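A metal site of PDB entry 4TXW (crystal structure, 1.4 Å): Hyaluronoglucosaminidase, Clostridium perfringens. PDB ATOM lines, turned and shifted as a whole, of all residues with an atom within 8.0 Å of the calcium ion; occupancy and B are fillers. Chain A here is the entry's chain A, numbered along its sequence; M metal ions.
The side-chain amino group (NZ) of Lys 24 lies close to the backbone carbonyl oxygen (O) of Arg 33, 3.5 Å away.
The side-chain carboxylate (OD1) of Asp 29 lies within hydrogen-bond range of the backbone NH (N) of Lys 31 (2.9 Å).
The side-chain amide nitrogen of Asn 156 is in hydrogen-bond range of the backbone carbonyl oxygen of Leu 30 (3.0 Å).
N of Asn 156 lies within hydrogen-bond range of O of Val 62, 2.9 Å away.
OE2 of Glu 157 sits at hydrogen-bond distance from N of Gly 28 (2.7 Å).
The backbone carbonyl oxygen (O) of Glu 157 is in hydrogen-bond range of the backbone NH (N) of Val 62 (2.9 Å).
Within 4 Å of the calcium ion: Lys 24, Asp 27, Asp 29, Thr 32, Asn 156 and Glu 157.
Along chain A the residues within 4 Å of the calcium ion span positions 24 to 157.
The nearest printed residue that does not touch the calcium ion is Leu 30 (4.4 Å).
The calcium ion is bound by the backbone carbonyl oxygen (O) of Lys 24, the backbone carbonyl oxygen (O) of Asp 29, the backbone carbonyl oxygen (O) of Asn 156, the side-chain carboxylate (OE1) of Glu 157, the side-chain hydroxyl (OG1) of Thr 32, the side-chain carboxylate (OD1) of Asp 27 and the backbone carbonyl oxygen (O) of Thr 32.
The calcium ion has seven donor atoms within binding distance.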
ATOM      1  N   GLY A  21      24.076 -26.315  22.781  1.00  0.00           N
ATOM      2  CA  GLY A  21      23.573 -27.421  23.572  1.00  0.00           C
ATOM      3  C   GLY A  21      22.216 -27.883  23.079  1.00  0.00           C
ATOM      4  O   GLY A  21      21.188 -27.543  23.661  1.00  0.00           O
ATOM      5  N   ALA A  22      22.219 -28.685  22.012  1.00  0.00           N
ATOM      6  CA  ALA A  22      20.998 -29.045  21.299  1.00  0.00           C
ATOM      7  C   ALA A  22      19.940 -29.766  22.123  1.00  0.00           C
ATOM      8  O   ALA A  22      18.764 -29.727  21.790  1.00  0.00           O
ATOM      9  CB  ALA A  22      21.350 -29.875  20.065  1.00  0.00           C
ATOM     10  N   LYS A  23      20.372 -30.426  23.203  1.00  0.00           N
ATOM     11  CA  LYS A  23      19.426 -31.126  24.080  1.00  0.00           C
ATOM     12  C   LYS A  23      18.366 -30.176  24.638  1.00  0.00           C
ATOM     13  O   LYS A  23      17.263 -30.592  24.965  1.00  0.00           O
ATOM     14  CB  LYS A  23      20.168 -31.813  25.246  1.00  0.00           C
ATOM     15  CG  LYS A  23      20.642 -30.837  26.324  1.00  0.00           C
ATOM     16  CD  LYS A  23      21.371 -31.540  27.478  1.00  0.00           C
ATOM     17  CE  LYS A  23      21.649 -30.564  28.633  1.00  0.00           C
ATOM     18  NZ  LYS A  23      22.234 -31.220  29.847  1.00  0.00           N
ATOM     19  N   LYS A  24      18.710 -28.889  24.737  1.00  0.00           N
ATOM     20  CA  LYS A  24      17.817 -27.920  25.350  1.00  0.00           C
ATOM     21  C   LYS A  24      16.518 -27.685  24.570  1.00  0.00           C
ATOM     22  O   LYS A  24      15.545 -27.175  25.111  1.00  0.00           O
ATOM     23  CB  LYS A  24      18.548 -26.605  25.647  1.00  0.00           C
ATOM     24  CG  LYS A  24      19.606 -26.784  26.754  1.00  0.00           C
ATOM     25  CD  LYS A  24      20.423 -25.512  26.981  1.00  0.00           C
ATOM     26  CE  LYS A  24      21.300 -25.197  25.782  1.00  0.00           C
ATOM     27  NZ  LYS A  24      22.322 -24.154  26.109  1.00  0.00           N
ATOM     28  N   ALA A  25      16.483 -28.106  23.311  1.00  0.00           N
ATOM     29  CA  ALA A  25      15.254 -27.985  22.520  1.00  0.00           C
ATOM     30  C   ALA A  25      14.229 -29.074  22.832  1.00  0.00           C
ATOM     31  O   ALA A  25      13.060 -28.945  22.482  1.00  0.00           O
ATOM     32  CB  ALA A  25      15.588 -28.019  21.050  1.00  0.00           C
ATOM     33  N   VAL A  26      14.670 -30.165  23.466  1.00  0.00           N
ATOM     34  CA  VAL A  26      13.824 -31.347  23.631  1.00  0.00           C
ATOM     35  C   VAL A  26      13.928 -31.917  25.039  1.00  0.00           C
ATOM     36  O   VAL A  26      13.770 -33.121  25.245  1.00  0.00           O
ATOM     37  CB  VAL A  26      14.181 -32.441  22.585  1.00  0.00           C
ATOM     38  CG1 VAL A  26      13.734 -32.014  21.193  1.00  0.00           C
ATOM     39  CG2 VAL A  26      15.683 -32.750  22.597  1.00  0.00           C
ATOM     40  N   ASP A  27      14.182 -31.046  26.008  1.00  0.00           N
ATOM     41  CA  ASP A  27      14.362 -31.486  27.397  1.00  0.00           C
ATOM     42  C   ASP A  27      13.099 -31.367  28.219  1.00  0.00           C
ATOM     43  O   ASP A  27      13.113 -31.693  29.407  1.00  0.00           O
ATOM     44  CB  ASP A  27      15.519 -30.747  28.085  1.00  0.00           C
ATOM     45  CG  ASP A  27      15.365 -29.239  28.070  1.00  0.00           C
ATOM     46  OD1 ASP A  27      14.328 -28.731  27.587  1.00  0.00           O
ATOM     47  OD2 ASP A  27      16.292 -28.540  28.551  1.00  0.00           O
ATOM     48  N   GLY A  28      12.018 -30.908  27.601  1.00  0.00           N
ATOM     49  CA  GLY A  28      10.740 -30.788  28.293  1.00  0.00           C
ATOM     50  C   GLY A  28      10.639 -29.558  29.164  1.00  0.00           C
ATOM     51  O   GLY A  28       9.677 -29.403  29.915  1.00  0.00           O
ATOM     52  N   ASP A  29      11.627 -28.673  29.055  1.00  0.00           N
ATOM     53  CA  ASP A  29      11.670 -27.462  29.875  1.00  0.00           C
ATOM     54  C   ASP A  29      11.547 -26.247  28.969  1.00  0.00           C
ATOM     55  O   ASP A  29      12.465 -25.945  28.212  1.00  0.00           O
ATOM     56  CB  ASP A  29      12.974 -27.430  30.678  1.00  0.00           C
ATOM     57  CG  ASP A  29      13.002 -26.320  31.705  1.00  0.00           C
ATOM     58  OD1 ASP A  29      12.291 -25.299  31.522  1.00  0.00           O
ATOM     59  OD2 ASP A  29      13.744 -26.457  32.712  1.00  0.00           O
ATOM     60  N   LEU A  30      10.425 -25.536  29.051  1.00  0.00           N
ATOM     61  CA  LEU A  30      10.193 -24.413  28.144  1.00  0.00           C
ATOM     62  C   LEU A  30      11.078 -23.212  28.455  1.00  0.00           C
ATOM     63  O   LEU A  30      11.123 -22.259  27.686  1.00  0.00           O
ATOM     64  CB  LEU A  30       8.708 -24.003  28.116  1.00  0.00           C
ATOM     65  CG  LEU A  30       7.632 -25.044  27.787  1.00  0.00           C
ATOM     66  CD1 LEU A  30       6.376 -24.391  27.203  1.00  0.00           C
ATOM     67  CD2 LEU A  30       8.142 -26.106  26.851  1.00  0.00           C
ATOM     68  N   LYS A  31      11.778 -23.241  29.583  1.00  0.00           N
ATOM     69  CA  LYS A  31      12.679 -22.142  29.942  1.00  0.00           C
ATOM     70  C   LYS A  31      14.110 -22.316  29.398  1.00  0.00           C
ATOM     71  O   LYS A  31      14.814 -21.332  29.174  1.00  0.00           O
ATOM     72  CB  LYS A  31      12.723 -21.958  31.465  1.00  0.00           C
ATOM     73  CG  LYS A  31      11.397 -21.523  32.071  1.00  0.00           C
ATOM     74  N   THR A  32      14.545 -23.557  29.194  1.00  0.00           N
ATOM     75  CA  THR A  32      15.866 -23.794  28.625  1.00  0.00           C
ATOM     76  C   THR A  32      15.812 -23.678  27.120  1.00  0.00           C
ATOM     77  O   THR A  32      14.833 -24.089  26.477  1.00  0.00           O
ATOM     78  CB  THR A  32      16.399 -25.188  28.961  1.00  0.00           C
ATOM     79  OG1 THR A  32      15.522 -26.167  28.398  1.00  0.00           O
ATOM     80  CG2 THR A  32      16.497 -25.374  30.481  1.00  0.00           C
ATOM     81  N   ARG A  33      16.863 -23.121  26.535  1.00  0.00           N
ATOM     82  CA  ARG A  33      16.854 -22.901  25.094  1.00  0.00           C
ATOM     83  C   ARG A  33      18.225 -23.135  24.484  1.00  0.00           C
ATOM     84  O   ARG A  33      19.245 -22.908  25.138  1.00  0.00           O
ATOM     85  CB  ARG A  33      16.360 -21.485  24.784  1.00  0.00           C
ATOM     86  CG  ARG A  33      17.287 -20.379  25.249  1.00  0.00           C
ATOM     87  CD  ARG A  33      16.511 -19.126  25.633  1.00  0.00           C
ATOM     88  NE  ARG A  33      17.403 -18.000  25.916  1.00  0.00           N
ATOM     89  CZ  ARG A  33      18.164 -17.902  27.007  1.00  0.00           C
ATOM     90  NH1 ARG A  33      18.934 -16.839  27.169  1.00  0.00           N
ATOM     91  NH2 ARG A  33      18.162 -18.865  27.925  1.00  0.00           N
ATOM     92  N   VAL A  34      18.224 -23.617  23.247  1.00  0.00           N
ATOM     93  CA  VAL A  34      19.432 -23.770  22.469  1.00  0.00           C
ATOM     94  C   VAL A  34      19.506 -22.712  21.388  1.00  0.00           C
ATOM     95  O   VAL A  34      18.492 -22.365  20.750  1.00  0.00           O
ATOM     96  CB  VAL A  34      19.570 -25.186  21.835  1.00  0.00           C
ATOM     97  CG1 VAL A  34      18.309 -25.586  21.057  1.00  0.00           C
ATOM     98  CG2 VAL A  34      20.810 -25.244  20.931  1.00  0.00           C
ATOM     99  N   VAL A  62       8.405 -23.228  20.548  1.00  0.00           N
ATOM    100  CA  VAL A  62       8.325 -22.190  21.581  1.00  0.00           C
ATOM    101  C   VAL A  62       9.632 -21.407  21.685  1.00  0.00           C
ATOM    102  O   VAL A  62      10.735 -21.993  21.642  1.00  0.00           O
ATOM    103  CB  VAL A  62       8.040 -22.833  22.955  1.00  0.00           C
ATOM    104  CG1 VAL A  62       7.905 -21.762  24.020  1.00  0.00           C
ATOM    105  CG2 VAL A  62       6.768 -23.678  22.905  1.00  0.00           C
ATOM    106  N   ILE A 155      15.740 -22.138  19.863  1.00  0.00           N
ATOM    107  CA  ILE A 155      14.598 -22.992  20.177  1.00  0.00           C
ATOM    108  C   ILE A 155      14.521 -23.208  21.676  1.00  0.00           C
ATOM    109  O   ILE A 155      15.441 -23.759  22.267  1.00  0.00           O
ATOM    110  CB  ILE A 155      14.730 -24.392  19.529  1.00  0.00           C
ATOM    111  CG1 ILE A 155      14.945 -24.295  18.026  1.00  0.00           C
ATOM    112  CG2 ILE A 155      13.477 -25.230  19.835  1.00  0.00           C
ATOM    113  CD1 ILE A 155      15.270 -25.635  17.369  1.00  0.00           C
ATOM    114  N   ASN A 156      13.423 -22.773  22.295  1.00  0.00           N
ATOM    115  CA  ASN A 156      13.197 -23.132  23.700  1.00  0.00           C
ATOM    116  C   ASN A 156      12.655 -24.560  23.786  1.00  0.00           C
ATOM    117  O   ASN A 156      13.080 -25.342  24.635  1.00  0.00           O
ATOM    118  CB  ASN A 156      12.240 -22.150  24.375  1.00  0.00           C
ATOM    119  CG  ASN A 156      12.907 -20.842  24.729  1.00  0.00           C
ATOM    120  OD1 ASN A 156      13.463 -20.155  23.862  1.00  0.00           O
ATOM    121  ND2 ASN A 156      12.856 -20.476  26.002  1.00  0.00           N
ATOM    122  N   GLU A 157      11.707 -24.906  22.917  1.00  0.00           N
ATOM    123  CA  GLU A 157      11.225 -26.276  22.887  1.00  0.00           C
ATOM    124  C   GLU A 157      10.535 -26.598  21.578  1.00  0.00           C
ATOM    125  O   GLU A 157       9.867 -25.750  20.992  1.00  0.00           O
ATOM    126  CB  GLU A 157      10.259 -26.546  24.057  1.00  0.00           C
ATOM    127  CG  GLU A 157      10.086 -28.025  24.422  1.00  0.00           C
ATOM    128  CD  GLU A 157      11.256 -28.604  25.201  1.00  0.00           C
ATOM    129  OE1 GLU A 157      12.064 -27.822  25.757  1.00  0.00           O
ATOM    130  OE2 GLU A 157      11.374 -29.836  25.247  1.00  0.00           O
ATOM    131  N   LEU A 158      10.745 -27.827  21.105  1.00  0.00           N
ATOM    132  CA  LEU A 158       9.853 -28.459  20.138  1.00  0.00           C
ATOM    133  C   LEU A 158       9.006 -29.388  20.965  1.00  0.00           C
ATOM    134  O   LEU A 158       9.440 -30.496  21.304  1.00  0.00           O
ATOM    135  CB  LEU A 158      10.658 -29.217  19.091  1.00  0.00           C
ATOM    136  CG  LEU A 158      11.464 -28.309  18.171  1.00  0.00           C
ATOM    137  CD1 LEU A 158      12.430 -29.098  17.299  1.00  0.00           C
ATOM    138  CD2 LEU A 158      10.539 -27.466  17.310  1.00  0.00           C
HETATM  139 CA    CA M   1      13.900 -26.468  26.508  1.00  0.00          CA
